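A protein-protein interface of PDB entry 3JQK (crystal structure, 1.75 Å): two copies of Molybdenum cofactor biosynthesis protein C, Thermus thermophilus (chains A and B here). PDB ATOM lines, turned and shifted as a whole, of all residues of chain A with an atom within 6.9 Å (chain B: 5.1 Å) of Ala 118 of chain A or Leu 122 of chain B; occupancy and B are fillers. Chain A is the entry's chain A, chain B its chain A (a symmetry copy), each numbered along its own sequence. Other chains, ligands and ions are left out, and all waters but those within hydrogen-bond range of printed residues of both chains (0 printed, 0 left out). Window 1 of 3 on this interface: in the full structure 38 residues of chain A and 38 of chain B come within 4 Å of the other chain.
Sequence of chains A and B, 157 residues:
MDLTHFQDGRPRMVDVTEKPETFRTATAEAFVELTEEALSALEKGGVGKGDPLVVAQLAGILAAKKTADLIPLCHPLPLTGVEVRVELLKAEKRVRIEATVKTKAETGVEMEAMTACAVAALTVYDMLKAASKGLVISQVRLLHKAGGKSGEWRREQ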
ATOM      1  N   GLU A  29     -36.476  32.053  16.495  1.00  0.00           N
ATOM      2  CA  GLU A  29     -35.953  33.257  15.878  1.00  0.00           C
ATOM      3  C   GLU A  29     -35.114  34.028  16.883  1.00  0.00           C
ATOM      4  O   GLU A  29     -35.188  33.787  18.089  1.00  0.00           O
ATOM      5  CB  GLU A  29     -37.097  34.141  15.354  1.00  0.00           C
ATOM      6  CG  GLU A  29     -37.696  35.099  16.364  1.00  0.00           C
ATOM      7  CD  GLU A  29     -38.875  35.884  15.805  1.00  0.00           C
ATOM      8  OE1 GLU A  29     -38.850  36.241  14.607  1.00  0.00           O
ATOM      9  OE2 GLU A  29     -39.821  36.149  16.570  1.00  0.00           O
ATOM     10  N   ALA A  30     -34.290  34.932  16.373  1.00  0.00           N
ATOM     11  CA  ALA A  30     -33.447  35.765  17.211  1.00  0.00           C
ATOM     12  C   ALA A  30     -33.219  37.070  16.460  1.00  0.00           C
ATOM     13  O   ALA A  30     -33.383  37.126  15.241  1.00  0.00           O
ATOM     14  CB  ALA A  30     -32.118  35.071  17.489  1.00  0.00           C
ATOM     15  N   ALA A  63     -24.399  24.875  14.023  1.00  0.00           N
ATOM     16  CA  ALA A  63     -24.767  24.895  15.439  1.00  0.00           C
ATOM     17  C   ALA A  63     -25.915  23.942  15.761  1.00  0.00           C
ATOM     18  O   ALA A  63     -25.925  23.297  16.810  1.00  0.00           O
ATOM     19  CB  ALA A  63     -25.130  26.312  15.861  1.00  0.00           C
ATOM     20  N   LEU A  70     -23.605  20.893  23.270  1.00  0.00           N
ATOM     21  CA  LEU A  70     -23.607  22.150  24.026  1.00  0.00           C
ATOM     22  C   LEU A  70     -24.595  22.202  25.188  1.00  0.00           C
ATOM     23  O   LEU A  70     -24.331  22.838  26.210  1.00  0.00           O
ATOM     24  CB  LEU A  70     -23.911  23.321  23.083  1.00  0.00           C
ATOM     25  CG  LEU A  70     -22.951  23.538  21.914  1.00  0.00           C
ATOM     26  CD1 LEU A  70     -23.505  24.618  20.989  1.00  0.00           C
ATOM     27  CD2 LEU A  70     -21.580  23.936  22.446  1.00  0.00           C
ATOM     28  N   ILE A  71     -25.739  21.550  25.017  1.00  0.00           N
ATOM     29  CA  ILE A  71     -26.780  21.527  26.038  1.00  0.00           C
ATOM     30  C   ILE A  71     -26.643  20.184  26.759  1.00  0.00           C
ATOM     31  O   ILE A  71     -26.999  19.134  26.216  1.00  0.00           O
ATOM     32  CB  ILE A  71     -28.165  21.661  25.374  1.00  0.00           C
ATOM     33  CG1 ILE A  71     -28.170  22.865  24.411  1.00  0.00           C
ATOM     34  CG2 ILE A  71     -29.238  21.796  26.434  1.00  0.00           C
ATOM     35  CD1 ILE A  71     -27.905  24.216  25.065  1.00  0.00           C
ATOM     36  N   ILE A  97     -33.013  36.510  12.509  1.00  0.00           N
ATOM     37  CA  ILE A  97     -32.577  35.151  12.234  1.00  0.00           C
ATOM     38  C   ILE A  97     -33.731  34.214  12.552  1.00  0.00           C
ATOM     39  O   ILE A  97     -34.393  34.354  13.583  1.00  0.00           O
ATOM     40  CB  ILE A  97     -31.358  34.750  13.103  1.00  0.00           C
ATOM     41  CG1 ILE A  97     -30.158  35.641  12.778  1.00  0.00           C
ATOM     42  CG2 ILE A  97     -30.999  33.290  12.856  1.00  0.00           C
ATOM     43  CD1 ILE A  97     -29.748  36.548  13.916  1.00  0.00           C
ATOM     44  N   GLU A 110     -36.637  21.619  19.749  1.00  0.00           N
ATOM     45  CA  GLU A 110     -36.725  23.023  20.104  1.00  0.00           C
ATOM     46  C   GLU A 110     -35.330  23.551  20.395  1.00  0.00           C
ATOM     47  O   GLU A 110     -34.990  24.661  19.997  1.00  0.00           O
ATOM     48  CB  GLU A 110     -37.610  23.225  21.335  1.00  0.00           C
ATOM     49  CG  GLU A 110     -39.046  22.798  21.122  1.00  0.00           C
ATOM     50  CD  GLU A 110     -39.326  21.397  21.618  1.00  0.00           C
ATOM     51  OE1 GLU A 110     -38.425  20.532  21.551  1.00  0.00           O
ATOM     52  OE2 GLU A 110     -40.464  21.159  22.069  1.00  0.00           O
ATOM     53  N   MET A 111     -34.514  22.751  21.077  1.00  0.00           N
ATOM     54  CA  MET A 111     -33.166  23.198  21.406  1.00  0.00           C
ATOM     55  C   MET A 111     -32.307  23.405  20.172  1.00  0.00           C
ATOM     56  O   MET A 111     -31.488  24.322  20.129  1.00  0.00           O
ATOM     57  CB  MET A 111     -32.479  22.219  22.364  1.00  0.00           C
ATOM     58  CG  MET A 111     -33.065  22.216  23.764  1.00  0.00           C
ATOM     59  SD  MET A 111     -33.472  23.881  24.369  1.00  0.00           S
ATOM     60  CE  MET A 111     -31.881  24.708  24.282  1.00  0.00           C
ATOM     61  N   ALA A 113     -33.380  24.325  17.206  1.00  0.00           N
ATOM     62  CA  ALA A 113     -33.823  25.558  16.559  1.00  0.00           C
ATOM     63  C   ALA A 113     -33.324  26.779  17.331  1.00  0.00           C
ATOM     64  O   ALA A 113     -32.818  27.735  16.745  1.00  0.00           O
ATOM     65  CB  ALA A 113     -35.346  25.587  16.469  1.00  0.00           C
ATOM     66  N   MET A 114     -33.472  26.742  18.649  1.00  0.00           N
ATOM     67  CA  MET A 114     -33.026  27.838  19.502  1.00  0.00           C
ATOM     68  C   MET A 114     -31.511  28.048  19.410  1.00  0.00           C
ATOM     69  O   MET A 114     -31.040  29.180  19.321  1.00  0.00           O
ATOM     70  CB  MET A 114     -33.412  27.559  20.957  1.00  0.00           C
ATOM     71  CG  MET A 114     -34.908  27.655  21.260  1.00  0.00           C
ATOM     72  SD  MET A 114     -35.513  29.356  21.256  1.00  0.00           S
ATOM     73  CE  MET A 114     -35.116  29.860  22.936  1.00  0.00           C
ATOM     74  N   THR A 115     -30.750  26.957  19.421  1.00  0.00           N
ATOM     75  CA  THR A 115     -29.295  27.056  19.362  1.00  0.00           C
ATOM     76  C   THR A 115     -28.805  27.555  18.005  1.00  0.00           C
ATOM     77  O   THR A 115     -27.842  28.311  17.932  1.00  0.00           O
ATOM     78  CB  THR A 115     -28.639  25.701  19.688  1.00  0.00           C
ATOM     79  OG1 THR A 115     -29.081  25.266  20.979  1.00  0.00           O
ATOM     80  CG2 THR A 115     -27.110  25.831  19.700  1.00  0.00           C
ATOM     81  N   ALA A 116     -29.464  27.132  16.932  1.00  0.00           N
ATOM     82  CA  ALA A 116     -29.088  27.584  15.600  1.00  0.00           C
ATOM     83  C   ALA A 116     -29.236  29.108  15.542  1.00  0.00           C
ATOM     84  O   ALA A 116     -28.356  29.810  15.043  1.00  0.00           O
ATOM     85  CB  ALA A 116     -29.981  26.915  14.545  1.00  0.00           C
ATOM     86  N   CYS A 117     -30.342  29.624  16.074  1.00  0.00           N
ATOM     87  CA  CYS A 117     -30.565  31.065  16.063  1.00  0.00           C
ATOM     88  C   CYS A 117     -29.571  31.813  16.937  1.00  0.00           C
ATOM     89  O   CYS A 117     -29.053  32.852  16.537  1.00  0.00           O
ATOM     90  CB  CYS A 117     -31.982  31.397  16.526  1.00  0.00           C
ATOM     91  SG  CYS A 117     -33.235  30.972  15.309  1.00  0.00           S
ATOM     92  N   ALA A 118     -29.306  31.279  18.125  1.00  0.00           N
ATOM     93  CA  ALA A 118     -28.379  31.922  19.053  1.00  0.00           C
ATOM     94  C   ALA A 118     -26.969  32.022  18.498  1.00  0.00           C
ATOM     95  O   ALA A 118     -26.326  33.063  18.612  1.00  0.00           O
ATOM     96  CB  ALA A 118     -28.356  31.174  20.383  1.00  0.00           C
ATOM     97  N   VAL A 119     -26.484  30.939  17.899  1.00  0.00           N
ATOM     98  CA  VAL A 119     -25.138  30.932  17.344  1.00  0.00           C
ATOM     99  C   VAL A 119     -25.040  31.796  16.086  1.00  0.00           C
ATOM    100  O   VAL A 119     -24.018  32.433  15.842  1.00  0.00           O
ATOM    101  CB  VAL A 119     -24.671  29.482  17.060  1.00  0.00           C
ATOM    102  CG1 VAL A 119     -23.311  29.493  16.385  1.00  0.00           C
ATOM    103  CG2 VAL A 119     -24.591  28.704  18.379  1.00  0.00           C
ATOM    104  N   ALA A 120     -26.099  31.834  15.283  1.00  0.00           N
ATOM    105  CA  ALA A 120     -26.070  32.679  14.096  1.00  0.00           C
ATOM    106  C   ALA A 120     -25.988  34.131  14.579  1.00  0.00           C
ATOM    107  O   ALA A 120     -25.253  34.944  14.021  1.00  0.00           O
ATOM    108  CB  ALA A 120     -27.327  32.459  13.253  1.00  0.00           C
ATOM    109  N   ALA A 121     -26.731  34.444  15.637  1.00  0.00           N
ATOM    110  CA  ALA A 121     -26.728  35.794  16.191  1.00  0.00           C
ATOM    111  C   ALA A 121     -25.339  36.130  16.730  1.00  0.00           C
ATOM    112  O   ALA A 121     -24.831  37.225  16.502  1.00  0.00           O
ATOM    113  CB  ALA A 121     -27.773  35.910  17.298  1.00  0.00           C
ATOM    114  N   LEU A 122     -24.729  35.182  17.437  1.00  0.00           N
ATOM    115  CA  LEU A 122     -23.385  35.386  17.979  1.00  0.00           C
ATOM    116  C   LEU A 122     -22.391  35.623  16.851  1.00  0.00           C
ATOM    117  O   LEU A 122     -21.429  36.374  17.009  1.00  0.00           O
ATOM    118  CB  LEU A 122     -22.938  34.164  18.797  1.00  0.00           C
ATOM    119  CG  LEU A 122     -23.578  33.992  20.176  1.00  0.00           C
ATOM    120  CD1 LEU A 122     -23.299  32.584  20.712  1.00  0.00           C
ATOM    121  CD2 LEU A 122     -23.026  35.041  21.124  1.00  0.00           C
ATOM    122  N   THR A 123     -22.619  34.983  15.708  1.00  0.00           N
ATOM    123  CA  THR A 123     -21.716  35.148  14.576  1.00  0.00           C
ATOM    124  C   THR A 123     -21.873  36.524  13.941  1.00  0.00           C
ATOM    125  O   THR A 123     -20.889  37.147  13.540  1.00  0.00           O
ATOM    126  CB  THR A 123     -21.931  34.033  13.545  1.00  0.00           C
ATOM    127  OG1 THR A 123     -21.623  32.780  14.163  1.00  0.00           O
ATOM    128  CG2 THR A 123     -21.018  34.227  12.338  1.00  0.00           C
ATOM    129  N   ILE A 137     -27.932  41.149  21.268  1.00  0.00           N
ATOM    130  CA  ILE A 137     -28.724  40.070  20.692  1.00  0.00           C
ATOM    131  C   ILE A 137     -29.950  40.231  21.587  1.00  0.00           C
ATOM    132  O   ILE A 137     -29.974  39.769  22.732  1.00  0.00           O
ATOM    133  CB  ILE A 137     -28.046  38.697  20.887  1.00  0.00           C
ATOM    134  CG1 ILE A 137     -26.790  38.627  20.010  1.00  0.00           C
ATOM    135  CG2 ILE A 137     -29.016  37.580  20.521  1.00  0.00           C
ATOM    136  CD1 ILE A 137     -25.913  37.398  20.255  1.00  0.00           C
ATOM    137  N   VAL A 140     -34.219  35.709  21.671  1.00  0.00           N
ATOM    138  CA  VAL A 140     -34.055  34.368  21.134  1.00  0.00           C
ATOM    139  C   VAL A 140     -35.280  33.693  21.716  1.00  0.00           C
ATOM    140  O   VAL A 140     -35.421  33.597  22.935  1.00  0.00           O
ATOM    141  CB  VAL A 140     -32.786  33.681  21.660  1.00  0.00           C
ATOM    142  CG1 VAL A 140     -32.596  32.354  20.944  1.00  0.00           C
ATOM    143  CG2 VAL A 140     -31.565  34.581  21.450  1.00  0.00           C
ATOM    144  N   CYS B 117     -22.489  33.052  27.965  1.00  0.00           N
ATOM    145  CA  CYS B 117     -23.786  33.533  28.425  1.00  0.00           C
ATOM    146  C   CYS B 117     -24.936  32.983  27.597  1.00  0.00           C
ATOM    147  O   CYS B 117     -25.958  32.581  28.146  1.00  0.00           O
ATOM    148  CB  CYS B 117     -23.839  35.059  28.398  1.00  0.00           C
ATOM    149  SG  CYS B 117     -22.850  35.819  29.692  1.00  0.00           S
ATOM    150  N   ALA B 118     -24.764  32.963  26.280  1.00  0.00           N
ATOM    151  CA  ALA B 118     -25.810  32.471  25.388  1.00  0.00           C
ATOM    152  C   ALA B 118     -26.141  31.008  25.623  1.00  0.00           C
ATOM    153  O   ALA B 118     -27.311  30.633  25.665  1.00  0.00           O
ATOM    154  CB  ALA B 118     -25.405  32.678  23.930  1.00  0.00           C
ATOM    155  N   VAL B 119     -25.114  30.179  25.775  1.00  0.00           N
ATOM    156  CA  VAL B 119     -25.328  28.756  25.995  1.00  0.00           C
ATOM    157  C   VAL B 119     -25.889  28.477  27.390  1.00  0.00           C
ATOM    158  O   VAL B 119     -26.696  27.568  27.569  1.00  0.00           O
ATOM    159  CB  VAL B 119     -24.020  27.961  25.753  1.00  0.00           C
ATOM    160  CG1 VAL B 119     -24.230  26.495  26.087  1.00  0.00           C
ATOM    161  CG2 VAL B 119     -23.599  28.106  24.286  1.00  0.00           C
ATOM    162  N   ALA B 120     -25.478  29.258  28.384  1.00  0.00           N
ATOM    163  CA  ALA B 120     -26.020  29.060  29.723  1.00  0.00           C
ATOM    164  C   ALA B 120     -27.513  29.394  29.658  1.00  0.00           C
ATOM    165  O   ALA B 120     -28.344  28.701  30.244  1.00  0.00           O
ATOM    166  CB  ALA B 120     -25.306  29.967  30.726  1.00  0.00           C
ATOM    167  N   ALA B 121     -27.852  30.447  28.920  1.00  0.00           N
ATOM    168  CA  ALA B 121     -29.245  30.855  28.777  1.00  0.00           C
ATOM    169  C   ALA B 121     -30.036  29.762  28.061  1.00  0.00           C
ATOM    170  O   ALA B 121     -31.146  29.428  28.468  1.00  0.00           O
ATOM    171  CB  ALA B 121     -29.332  32.169  28.006  1.00  0.00           C
ATOM    172  N   LEU B 122     -29.455  29.205  27.002  1.00  0.00           N
ATOM    173  CA  LEU B 122     -30.109  28.129  26.256  1.00  0.00           C
ATOM    174  C   LEU B 122     -30.337  26.924  27.157  1.00  0.00           C
ATOM    175  O   LEU B 122     -31.324  26.205  27.006  1.00  0.00           O
ATOM    176  CB  LEU B 122     -29.253  27.704  25.052  1.00  0.00           C
ATOM    177  CG  LEU B 122     -29.232  28.658  23.856  1.00  0.00           C
ATOM    178  CD1 LEU B 122     -28.096  28.278  22.901  1.00  0.00           C
ATOM    179  CD2 LEU B 122     -30.570  28.602  23.141  1.00  0.00           C
ATOM    180  N   THR B 123     -29.424  26.698  28.098  1.00  0.00           N
ATOM    181  CA  THR B 123     -29.561  25.564  29.002  1.00  0.00           C
ATOM    182  C   THR B 123     -30.676  25.797  30.014  1.00  0.00           C
ATOM    183  O   THR B 123     -31.425  24.877  30.345  1.00  0.00           O
ATOM    184  CB  THR B 123     -28.229  25.268  29.703  1.00  0.00           C
ATOM    185  OG1 THR B 123     -27.264  24.912  28.708  1.00  0.00           O
ATOM    186  CG2 THR B 123     -28.379  24.108  30.684  1.00  0.00           C
ATOM    187  N   VAL B 124     -30.797  27.027  30.500  1.00  0.00           N
ATOM    188  CA  VAL B 124     -31.874  27.348  31.427  1.00  0.00           C
ATOM    189  C   VAL B 124     -33.183  27.085  30.680  1.00  0.00           C
ATOM    190  O   VAL B 124     -34.116  26.495  31.226  1.00  0.00           O
ATOM    191  CB  VAL B 124     -31.828  28.831  31.856  1.00  0.00           C
ATOM    192  CG1 VAL B 124     -33.122  29.207  32.591  1.00  0.00           C
ATOM    193  CG2 VAL B 124     -30.630  29.072  32.756  1.00  0.00           C
ATOM    194  N   TYR B 125     -33.245  27.525  29.424  1.00  0.00           N
ATOM    195  CA  TYR B 125     -34.441  27.320  28.615  1.00  0.00           C
ATOM    196  C   TYR B 125     -34.716  25.820  28.471  1.00  0.00           C
ATOM    197  O   TYR B 125     -35.848  25.367  28.627  1.00  0.00           O
ATOM    198  CB  TYR B 125     -34.264  27.948  27.223  1.00  0.00           C
ATOM    199  CG  TYR B 125     -35.443  27.701  26.306  1.00  0.00           C
ATOM    200  CD1 TYR B 125     -36.612  28.451  26.422  1.00  0.00           C
ATOM    201  CD2 TYR B 125     -35.409  26.677  25.362  1.00  0.00           C
ATOM    202  CE1 TYR B 125     -37.727  28.181  25.615  1.00  0.00           C
ATOM    203  CE2 TYR B 125     -36.509  26.399  24.555  1.00  0.00           C
ATOM    204  CZ  TYR B 125     -37.665  27.153  24.688  1.00  0.00           C
ATOM    205  OH  TYR B 125     -38.764  26.857  23.909  1.00  0.00           O
ATOM    206  N   ASP B 126     -33.673  25.045  28.183  1.00  0.00           N
ATOM    207  CA  ASP B 126     -33.849  23.605  28.018  1.00  0.00           C
ATOM    208  C   ASP B 126     -34.463  22.951  29.251  1.00  0.00           C
ATOM    209  O   ASP B 126     -35.327  22.078  29.132  1.00  0.00           O
ATOM    210  CB  ASP B 126     -32.506  22.926  27.719  1.00  0.00           C
ATOM    211  CG  ASP B 126     -32.641  21.416  27.577  1.00  0.00           C
ATOM    212  OD1 ASP B 126     -33.419  20.979  26.709  1.00  0.00           O
ATOM    213  OD2 ASP B 126     -31.976  20.670  28.330  1.00  0.00           O
ATOM    214  N   ILE B 137     -35.099  34.422  25.789  1.00  0.00           N
ATOM    215  CA  ILE B 137     -33.753  34.802  26.202  1.00  0.00           C
ATOM    216  C   ILE B 137     -33.789  36.236  25.681  1.00  0.00           C
ATOM    217  O   ILE B 137     -33.601  36.490  24.486  1.00  0.00           O
ATOM    218  CB  ILE B 137     -32.676  33.957  25.487  1.00  0.00           C
ATOM    219  CG1 ILE B 137     -32.738  32.516  26.011  1.00  0.00           C
ATOM    220  CG2 ILE B 137     -31.296  34.555  25.733  1.00  0.00           C
ATOM    221  CD1 ILE B 137     -31.859  31.525  25.246  1.00  0.00           C
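The backbone carbonyl oxygen of Ile 137 of chain B is in hydrogen-bond range of the backbone NH of Val 140 of chain A (3.0 Å). SD of Met 111 of chain A lies close to OD1 of Asp 126 of chain B, 3.7 Å away.
The backbone carbonyl oxygen of Met 111 of chain A sits at hydrogen-bond distance from the side-chain hydroxyl of Thr 115 of chain A (2.7 Å). The backbone carbonyl oxygen (O) of Val 119 of chain B is in hydrogen-bond range of the side-chain hydroxyl (OG1) of Thr 123 of chain B, at 2.9 Å.
Among the printed residues, pairs that only touch across the chains: Leu 70 of chain A with Val 119 of chain B (3.7 Å), Ile 71 of chain A with Leu 122 of chain B (3.7 Å), Ile 71 of chain A with Thr 123 of chain B (3.8 Å), Ile 71 of chain A with Asp 126 of chain B (3.5 Å), Met 111 of chain A with Leu 122 of chain B (3.2 Å), Met 111 of chain A with Tyr 125 of chain B (3.5 Å), Met 114 of chain A with Leu 122 of chain B (3.7 Å), Met 114 of chain A with Tyr 125 of chain B (3.9 Å), Thr 115 of chain A with Leu 122 of chain B (3.7 Å), Ala 118 of chain A with Leu 122 of chain B (3.8 Å) and Leu 122 of chain A with Ala 118 of chain B (3.8 Å).
Printed residues of chain B within 4 Å of Met 111 of chain A: Leu 122, Tyr 125 and Asp 126. Ala 116 of chain A touches none of the printed residues of chain B. Printed residues of chain B within 4 Å of Val 140 of chain A: Ile 137 (3.0 Å). Of the printed residues of chain A, Ala 118 of chain B touches Leu 122 (3.8 Å). Leu 122 of chain B touches five residues of chain A. Printed residues of chain A within 4 Å of Tyr 125 of chain B: Met 111 and Met 114. Printed residues of chain A within 4 Å of Asp 126 of chain B: Ile 71 and Met 111. The nearest residue of chain B that does not touch Ala 118 of chain A is Ala 118 of chain B (4.9 Å). The nearest printed residue of chain B that does not touch Ile 71 of chain A is Val 119 of chain B (4.4 Å).
Of the 21 printed residues of chain A, 8 touch a printed residue of chain B. Printed residues of chain B that touch a printed residue of chain A: Ala 118, Val 119, Leu 122, Thr 123, Tyr 125, Asp 126 and Ile 137. Hydrophobic or aromatic side chains of chain B that line the printed part of chain A: Ala 118, Val 119, Leu 122, Tyr 125 and Ile 137. Among the printed residues, 13 pairs touch across the chains. Among the printed residues, no Asp or Glu carboxylate lies within 4 Å of a Lys or Arg side-chain nitrogen of the other chain.
Ala 118 of chain A touches Leu 122 of chain B, and with the chains exchanged Leu 122 of chain A touches Ala 118 of chain B. Positions printed for both chains: 117, 118, 119, 120, 121, 122, 123 and 137. Of the 13 pairs that touch across the chains among the printed residues, 2 have their exchanged pair printed and touching as well.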
